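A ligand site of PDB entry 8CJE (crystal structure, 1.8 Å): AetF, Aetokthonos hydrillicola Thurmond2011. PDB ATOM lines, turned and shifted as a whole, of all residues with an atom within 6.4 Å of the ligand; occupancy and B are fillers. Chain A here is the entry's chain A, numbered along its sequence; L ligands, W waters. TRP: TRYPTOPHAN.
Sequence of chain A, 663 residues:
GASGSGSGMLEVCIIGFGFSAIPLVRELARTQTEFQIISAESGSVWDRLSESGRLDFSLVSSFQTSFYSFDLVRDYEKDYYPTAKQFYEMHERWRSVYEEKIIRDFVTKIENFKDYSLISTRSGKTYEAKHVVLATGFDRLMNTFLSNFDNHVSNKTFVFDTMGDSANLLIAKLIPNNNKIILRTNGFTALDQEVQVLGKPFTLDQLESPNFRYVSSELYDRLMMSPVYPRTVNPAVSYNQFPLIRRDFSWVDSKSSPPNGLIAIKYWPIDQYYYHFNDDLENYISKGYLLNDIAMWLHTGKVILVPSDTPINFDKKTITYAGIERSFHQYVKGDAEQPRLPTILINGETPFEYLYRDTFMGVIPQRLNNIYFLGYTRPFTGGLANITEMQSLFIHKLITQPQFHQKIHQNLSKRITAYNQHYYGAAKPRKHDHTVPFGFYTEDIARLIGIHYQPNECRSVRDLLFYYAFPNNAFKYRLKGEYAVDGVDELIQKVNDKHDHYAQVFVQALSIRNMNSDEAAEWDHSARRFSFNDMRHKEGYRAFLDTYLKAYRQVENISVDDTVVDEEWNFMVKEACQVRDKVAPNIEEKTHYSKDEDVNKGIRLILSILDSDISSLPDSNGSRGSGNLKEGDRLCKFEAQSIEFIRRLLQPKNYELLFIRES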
ATOM      1  N   LEU A 191       1.431 -31.837   0.577  1.00  0.00           N
ATOM      2  CA  LEU A 191       0.425 -32.319   1.512  1.00  0.00           C
ATOM      3  C   LEU A 191       0.035 -33.755   1.214  1.00  0.00           C
ATOM      4  O   LEU A 191      -0.232 -34.090   0.048  1.00  0.00           O
ATOM      5  CB  LEU A 191      -0.837 -31.445   1.464  1.00  0.00           C
ATOM      6  CG  LEU A 191      -0.643 -29.987   1.826  1.00  0.00           C
ATOM      7  CD1 LEU A 191      -1.889 -29.211   1.466  1.00  0.00           C
ATOM      8  CD2 LEU A 191      -0.370 -29.858   3.301  1.00  0.00           C
ATOM      9  N   VAL A 195      -4.943 -38.778   4.811  1.00  0.00           N
ATOM     10  CA  VAL A 195      -4.472 -38.733   6.186  1.00  0.00           C
ATOM     11  C   VAL A 195      -5.321 -39.685   7.026  1.00  0.00           C
ATOM     12  O   VAL A 195      -6.302 -40.254   6.566  1.00  0.00           O
ATOM     13  CB  VAL A 195      -4.521 -37.302   6.782  1.00  0.00           C
ATOM     14  CG1 VAL A 195      -3.845 -36.329   5.848  1.00  0.00           C
ATOM     15  CG2 VAL A 195      -5.942 -36.895   7.018  1.00  0.00           C
ATOM     16  N   LEU A 204      -7.825 -35.596   1.966  1.00  0.00           N
ATOM     17  CA  LEU A 204      -7.618 -34.304   2.619  1.00  0.00           C
ATOM     18  C   LEU A 204      -8.770 -33.338   2.363  1.00  0.00           C
ATOM     19  O   LEU A 204      -9.088 -32.532   3.231  1.00  0.00           O
ATOM     20  CB  LEU A 204      -6.278 -33.707   2.178  1.00  0.00           C
ATOM     21  CG  LEU A 204      -6.179 -32.905   0.870  1.00  0.00           C
ATOM     22  CD1 LEU A 204      -4.911 -32.094   0.865  1.00  0.00           C
ATOM     23  CD2 LEU A 204      -6.248 -33.833  -0.339  1.00  0.00           C
ATOM     24  N   ASP A 205      -9.395 -33.400   1.195  1.00  0.00           N
ATOM     25  CA  ASP A 205     -10.538 -32.537   0.881  1.00  0.00           C
ATOM     26  C   ASP A 205     -11.708 -32.765   1.817  1.00  0.00           C
ATOM     27  O   ASP A 205     -12.624 -31.939   1.837  1.00  0.00           O
ATOM     28  CB  ASP A 205     -11.008 -32.771  -0.555  1.00  0.00           C
ATOM     29  CG  ASP A 205     -11.156 -34.240  -0.892  1.00  0.00           C
ATOM     30  OD1 ASP A 205     -10.119 -34.922  -1.039  1.00  0.00           O
ATOM     31  OD2 ASP A 205     -12.293 -34.730  -0.964  1.00  0.00           O
ATOM     32  N   LEU A 207     -11.585 -32.714   5.017  1.00  0.00           N
ATOM     33  CA  LEU A 207     -11.268 -32.186   6.331  1.00  0.00           C
ATOM     34  C   LEU A 207     -11.060 -30.684   6.291  1.00  0.00           C
ATOM     35  O   LEU A 207     -10.359 -30.116   7.137  1.00  0.00           O
ATOM     36  CB  LEU A 207     -10.038 -32.883   6.897  1.00  0.00           C
ATOM     37  CG  LEU A 207      -9.971 -34.422   6.881  1.00  0.00           C
ATOM     38  CD1 LEU A 207      -8.664 -34.865   7.461  1.00  0.00           C
ATOM     39  CD2 LEU A 207     -11.101 -35.052   7.633  1.00  0.00           C
ATOM     40  N   GLU A 208     -11.714 -30.004   5.359  1.00  0.00           N
ATOM     41  CA  GLU A 208     -11.495 -28.573   5.209  1.00  0.00           C
ATOM     42  C   GLU A 208     -12.598 -27.707   5.793  1.00  0.00           C
ATOM     43  O   GLU A 208     -12.322 -26.538   6.070  1.00  0.00           O
ATOM     44  CB  GLU A 208     -11.300 -28.238   3.737  1.00  0.00           C
ATOM     45  CG  GLU A 208     -10.125 -28.968   3.203  1.00  0.00           C
ATOM     46  CD  GLU A 208      -9.809 -28.561   1.815  1.00  0.00           C
ATOM     47  OE1 GLU A 208     -10.202 -27.443   1.412  1.00  0.00           O
ATOM     48  OE2 GLU A 208      -9.153 -29.362   1.110  1.00  0.00           O
ATOM     49  N   SER A 209     -13.800 -28.243   5.998  1.00  0.00           N
ATOM     50  CA  SER A 209     -14.985 -27.595   6.596  1.00  0.00           C
ATOM     51  C   SER A 209     -14.990 -26.087   6.363  1.00  0.00           C
ATOM     52  O   SER A 209     -14.942 -25.321   7.330  1.00  0.00           O
ATOM     53  CB  SER A 209     -15.062 -27.856   8.089  1.00  0.00           C
ATOM     54  OG  SER A 209     -13.904 -27.383   8.750  1.00  0.00           O
ATOM     55  N   ARG A 222      -6.343 -20.758  11.911  1.00  0.00           N
ATOM     56  CA  ARG A 222      -5.732 -21.723  12.825  1.00  0.00           C
ATOM     57  C   ARG A 222      -6.085 -23.147  12.443  1.00  0.00           C
ATOM     58  O   ARG A 222      -5.312 -24.071  12.731  1.00  0.00           O
ATOM     59  CB  ARG A 222      -6.171 -21.417  14.256  1.00  0.00           C
ATOM     60  CG  ARG A 222      -5.747 -20.056  14.710  1.00  0.00           C
ATOM     61  CD  ARG A 222      -5.857 -19.919  16.217  1.00  0.00           C
ATOM     62  NE  ARG A 222      -7.231 -20.112  16.663  1.00  0.00           N
ATOM     63  CZ  ARG A 222      -8.119 -19.133  16.724  1.00  0.00           C
ATOM     64  NH1 ARG A 222      -7.816 -17.899  16.370  1.00  0.00           N
ATOM     65  NH2 ARG A 222      -9.353 -19.403  17.146  1.00  0.00           N
ATOM     66  N   LEU A 223      -7.226 -23.337  11.776  1.00  0.00           N
ATOM     67  CA  LEU A 223      -7.658 -24.659  11.379  1.00  0.00           C
ATOM     68  C   LEU A 223      -6.834 -25.242  10.240  1.00  0.00           C
ATOM     69  O   LEU A 223      -6.769 -26.467  10.090  1.00  0.00           O
ATOM     70  CB  LEU A 223      -9.129 -24.624  10.938  1.00  0.00           C
ATOM     71  CG  LEU A 223     -10.239 -24.630  11.981  1.00  0.00           C
ATOM     72  CD1 LEU A 223     -11.587 -24.389  11.345  1.00  0.00           C
ATOM     73  CD2 LEU A 223     -10.239 -25.950  12.673  1.00  0.00           C
ATOM     74  N   MET A 224      -6.159 -24.397   9.449  1.00  0.00           N
ATOM     75  CA  MET A 224      -5.621 -24.864   8.174  1.00  0.00           C
ATOM     76  C   MET A 224      -4.153 -24.561   7.923  1.00  0.00           C
ATOM     77  O   MET A 224      -3.529 -25.292   7.161  1.00  0.00           O
ATOM     78  CB  MET A 224      -6.438 -24.281   7.015  1.00  0.00           C
ATOM     79  CG  MET A 224      -7.892 -24.629   7.075  1.00  0.00           C
ATOM     80  SD  MET A 224      -8.290 -26.265   6.462  1.00  0.00           S
ATOM     81  CE  MET A 224      -8.006 -26.089   4.713  1.00  0.00           C
ATOM     82  N   MET A 225      -3.566 -23.531   8.533  1.00  0.00           N
ATOM     83  CA  MET A 225      -2.317 -23.025   7.990  1.00  0.00           C
ATOM     84  C   MET A 225      -1.058 -23.510   8.697  1.00  0.00           C
ATOM     85  O   MET A 225       0.021 -23.348   8.141  1.00  0.00           O
ATOM     86  CB  MET A 225      -2.323 -21.498   7.992  1.00  0.00           C
ATOM     87  CG  MET A 225      -3.465 -20.910   7.201  1.00  0.00           C
ATOM     88  SD  MET A 225      -3.574 -21.618   5.556  1.00  0.00           S
ATOM     89  CE  MET A 225      -2.130 -20.929   4.755  1.00  0.00           C
ATOM     90  N   SER A 226      -1.164 -24.138   9.875  1.00  0.00           N
ATOM     91  CA  SER A 226       0.050 -24.610  10.519  1.00  0.00           C
ATOM     92  C   SER A 226       0.803 -25.676   9.720  1.00  0.00           C
ATOM     93  O   SER A 226       2.039 -25.745   9.862  1.00  0.00           O
ATOM     94  CB  SER A 226      -0.262 -25.105  11.939  1.00  0.00           C
ATOM     95  OG  SER A 226      -0.592 -26.467  11.950  1.00  0.00           O
ATOM     96  N   PRO A 227       0.170 -26.494   8.860  1.00  0.00           N
ATOM     97  CA  PRO A 227       0.961 -27.357   7.964  1.00  0.00           C
ATOM     98  C   PRO A 227       1.581 -26.629   6.789  1.00  0.00           C
ATOM     99  O   PRO A 227       2.399 -27.224   6.078  1.00  0.00           O
ATOM    100  CB  PRO A 227      -0.060 -28.391   7.471  1.00  0.00           C
ATOM    101  CG  PRO A 227      -1.158 -28.357   8.481  1.00  0.00           C
ATOM    102  CD  PRO A 227      -1.240 -26.915   8.884  1.00  0.00           C
ATOM    103  N   VAL A 228       1.219 -25.375   6.543  1.00  0.00           N
ATOM    104  CA  VAL A 228       1.742 -24.617   5.415  1.00  0.00           C
ATOM    105  C   VAL A 228       2.744 -23.574   5.878  1.00  0.00           C
ATOM    106  O   VAL A 228       3.867 -23.523   5.383  1.00  0.00           O
ATOM    107  CB  VAL A 228       0.586 -23.969   4.597  1.00  0.00           C
ATOM    108  CG1 VAL A 228       1.149 -23.194   3.401  1.00  0.00           C
ATOM    109  CG2 VAL A 228      -0.380 -25.010   4.132  1.00  0.00           C
ATOM    110  N   PRO A 258      -6.960 -20.298   3.522  1.00  0.00           N
ATOM    111  CA  PRO A 258      -5.732 -20.307   2.711  1.00  0.00           C
ATOM    112  C   PRO A 258      -5.836 -19.273   1.608  1.00  0.00           C
ATOM    113  O   PRO A 258      -6.891 -19.087   1.029  1.00  0.00           O
ATOM    114  CB  PRO A 258      -5.680 -21.741   2.177  1.00  0.00           C
ATOM    115  CG  PRO A 258      -7.049 -22.263   2.320  1.00  0.00           C
ATOM    116  CD  PRO A 258      -7.600 -21.623   3.516  1.00  0.00           C
ATOM    117  N   PHE A 380      -7.476 -25.226  -5.087  1.00  0.00           N
ATOM    118  CA  PHE A 380      -6.297 -25.464  -4.266  1.00  0.00           C
ATOM    119  C   PHE A 380      -6.185 -26.937  -3.888  1.00  0.00           C
ATOM    120  O   PHE A 380      -5.093 -27.507  -3.938  1.00  0.00           O
ATOM    121  CB  PHE A 380      -6.341 -24.573  -3.024  1.00  0.00           C
ATOM    122  CG  PHE A 380      -5.346 -24.926  -1.954  1.00  0.00           C
ATOM    123  CD1 PHE A 380      -3.999 -24.965  -2.223  1.00  0.00           C
ATOM    124  CD2 PHE A 380      -5.766 -25.156  -0.671  1.00  0.00           C
ATOM    125  CE1 PHE A 380      -3.106 -25.258  -1.237  1.00  0.00           C
ATOM    126  CE2 PHE A 380      -4.867 -25.461   0.318  1.00  0.00           C
ATOM    127  CZ  PHE A 380      -3.544 -25.508   0.032  1.00  0.00           C
ATOM    128  N   THR A 381      -7.306 -27.581  -3.532  1.00  0.00           N
ATOM    129  CA  THR A 381      -7.373 -29.013  -3.296  1.00  0.00           C
ATOM    130  C   THR A 381      -8.567 -29.614  -4.016  1.00  0.00           C
ATOM    131  O   THR A 381      -9.540 -28.930  -4.335  1.00  0.00           O
ATOM    132  CB  THR A 381      -7.505 -29.320  -1.808  1.00  0.00           C
ATOM    133  OG1 THR A 381      -8.652 -28.644  -1.294  1.00  0.00           O
ATOM    134  CG2 THR A 381      -6.277 -28.875  -1.061  1.00  0.00           C
ATOM    135  N   VAL A 505     -14.261 -33.482  11.885  1.00  0.00           N
ATOM    136  CA  VAL A 505     -13.768 -32.177  11.467  1.00  0.00           C
ATOM    137  C   VAL A 505     -14.412 -31.064  12.292  1.00  0.00           C
ATOM    138  O   VAL A 505     -13.764 -30.074  12.645  1.00  0.00           O
ATOM    139  CB  VAL A 505     -14.023 -31.970   9.963  1.00  0.00           C
ATOM    140  CG1 VAL A 505     -13.400 -30.682   9.517  1.00  0.00           C
ATOM    141  CG2 VAL A 505     -13.458 -33.113   9.199  1.00  0.00           C
ATOM    142  N   GLN A 508     -12.591 -30.573  15.455  1.00  0.00           N
ATOM    143  CA  GLN A 508     -11.325 -29.868  15.364  1.00  0.00           C
ATOM    144  C   GLN A 508     -11.495 -28.389  15.651  1.00  0.00           C
ATOM    145  O   GLN A 508     -10.705 -27.790  16.372  1.00  0.00           O
ATOM    146  CB  GLN A 508     -10.693 -30.062  13.991  1.00  0.00           C
ATOM    147  CG  GLN A 508      -9.303 -29.487  13.939  1.00  0.00           C
ATOM    148  CD  GLN A 508      -8.841 -29.222  12.551  1.00  0.00           C
ATOM    149  OE1 GLN A 508      -9.381 -29.754  11.577  1.00  0.00           O
ATOM    150  NE2 GLN A 508      -7.856 -28.349  12.418  1.00  0.00           N
ATOM    151  N   ASP A 524      -1.824 -29.195  16.557  1.00  0.00           N
ATOM    152  CA  ASP A 524      -1.947 -29.954  15.321  1.00  0.00           C
ATOM    153  C   ASP A 524      -0.906 -31.063  15.255  1.00  0.00           C
ATOM    154  O   ASP A 524      -1.178 -32.158  14.754  1.00  0.00           O
ATOM    155  CB  ASP A 524      -1.770 -29.036  14.111  1.00  0.00           C
ATOM    156  CG  ASP A 524      -2.907 -28.091  13.913  1.00  0.00           C
ATOM    157  OD1 ASP A 524      -4.043 -28.405  14.341  1.00  0.00           O
ATOM    158  OD2 ASP A 524      -2.658 -26.994  13.365  1.00  0.00           O
ATOM    159  N   SER A 531      -1.565 -34.790  10.457  1.00  0.00           N
ATOM    160  CA  SER A 531      -2.105 -34.946   9.116  1.00  0.00           C
ATOM    161  C   SER A 531      -1.030 -34.889   8.052  1.00  0.00           C
ATOM    162  O   SER A 531      -0.992 -35.725   7.163  1.00  0.00           O
ATOM    163  CB  SER A 531      -3.166 -33.872   8.834  1.00  0.00           C
ATOM    164  OG  SER A 531      -4.303 -34.006   9.663  1.00  0.00           O
ATOM    165  N   PHE A 532      -0.120 -33.931   8.149  1.00  0.00           N
ATOM    166  CA  PHE A 532       0.742 -33.635   7.015  1.00  0.00           C
ATOM    167  C   PHE A 532       2.216 -33.656   7.390  1.00  0.00           C
ATOM    168  O   PHE A 532       2.630 -33.020   8.371  1.00  0.00           O
ATOM    169  CB  PHE A 532       0.377 -32.290   6.406  1.00  0.00           C
ATOM    170  CG  PHE A 532      -1.088 -32.187   6.006  1.00  0.00           C
ATOM    171  CD1 PHE A 532      -1.588 -32.946   4.961  1.00  0.00           C
ATOM    172  CD2 PHE A 532      -1.922 -31.279   6.622  1.00  0.00           C
ATOM    173  CE1 PHE A 532      -2.912 -32.847   4.583  1.00  0.00           C
ATOM    174  CE2 PHE A 532      -3.253 -31.167   6.241  1.00  0.00           C
ATOM    175  CZ  PHE A 532      -3.742 -31.946   5.231  1.00  0.00           C
ATOM    176  N   LYS A 595      -3.869 -34.071  20.710  1.00  0.00           N
ATOM    177  CA  LYS A 595      -4.879 -33.990  19.656  1.00  0.00           C
ATOM    178  C   LYS A 595      -5.738 -35.238  19.592  1.00  0.00           C
ATOM    179  O   LYS A 595      -6.954 -35.169  19.397  1.00  0.00           O
ATOM    180  CB  LYS A 595      -4.232 -33.721  18.292  1.00  0.00           C
ATOM    181  CG  LYS A 595      -5.234 -33.840  17.142  1.00  0.00           C
ATOM    182  CD  LYS A 595      -4.697 -33.323  15.806  1.00  0.00           C
ATOM    183  CE  LYS A 595      -5.738 -33.429  14.709  1.00  0.00           C
ATOM    184  NZ  LYS A 595      -5.211 -33.097  13.368  1.00  0.00           N
HETATM  185  N   TRP L   1      -8.187 -29.256   9.044  1.00  0.00           N
HETATM  186  CA  TRP L   1      -7.554 -30.526   8.788  1.00  0.00           C
HETATM  187  C   TRP L   1      -6.312 -30.684   9.641  1.00  0.00           C
HETATM  188  O   TRP L   1      -5.939 -29.747  10.352  1.00  0.00           O
HETATM  189  CB  TRP L   1      -7.224 -30.656   7.303  1.00  0.00           C
HETATM  190  CG  TRP L   1      -6.290 -29.608   6.737  1.00  0.00           C
HETATM  191  CD1 TRP L   1      -5.426 -28.788   7.434  1.00  0.00           C
HETATM  192  CD2 TRP L   1      -6.125 -29.273   5.345  1.00  0.00           C
HETATM  193  NE1 TRP L   1      -4.747 -27.980   6.561  1.00  0.00           N
HETATM  194  CE2 TRP L   1      -5.151 -28.256   5.277  1.00  0.00           C
HETATM  195  CE3 TRP L   1      -6.693 -29.736   4.172  1.00  0.00           C
HETATM  196  CZ2 TRP L   1      -4.752 -27.697   4.079  1.00  0.00           C
HETATM  197  CZ3 TRP L   1      -6.293 -29.183   2.982  1.00  0.00           C
HETATM  198  CH2 TRP L   1      -5.323 -28.179   2.943  1.00  0.00           C
HETATM  199  OXT TRP L   1      -5.642 -31.724   9.604  1.00  0.00           O
HETATM  200  O   HOH W   1      -5.567 -30.336  13.157  1.00  0.00           O
HETATM  201  O   HOH W   2     -10.586 -27.399   8.867  1.00  0.00           O
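An oxygen (OXT) of the ligand sits at hydrogen-bond distance from the side-chain hydroxyl (OG) of Ser 531 (2.6 Å). OE1 of Gln 508 lies within hydrogen-bond range of N of the ligand (2.8 Å). The backbone carbonyl oxygen of Met 224 is in hydrogen-bond range of a nitrogen (NE1) of the ligand (3.0 Å). O of Leu 207 is in hydrogen-bond range of N of the ligand (3.0 Å). The backbone carbonyl oxygen (O) of Leu 223 sits at hydrogen-bond distance from a nitrogen (N) of the ligand (3.3 Å).
The backbone carbonyl oxygen (O) of Leu 223 is in hydrogen-bond range of the side-chain amide nitrogen (NE2) of Gln 508, 3.2 Å away. The side-chain carboxylate (OE2) of Glu 208 lies within hydrogen-bond range of the side-chain hydroxyl (OG1) of Thr 381, at 2.6 Å.
Leu 191 touches the ligand. O of Leu 204 touches CE3 of the ligand (3.8 Å). OE2 of Glu 208 touches CZ3 of the ligand, 3.4 Å away. Phe 380 touches the ligand (CE2 to CH2, 3.8 Å). CE2 of Phe 532 touches CD1 of the ligand (3.4 Å). Within 4 Å of the ligand: Leu 191, Leu 204, Leu 207, Glu 208, Leu 223, Met 224, Phe 380, Gln 508, Ser 531 and Phe 532. Along chain A the residues within 4 Å of the ligand span positions 191 to 532.
Water W1 lies within hydrogen-bond range of OD1 of Asp 524 (2.7 Å), NZ of Lys 595 (2.8 Å), O of the ligand (2.9 Å) and NE2 of Gln 508 (3.1 Å).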
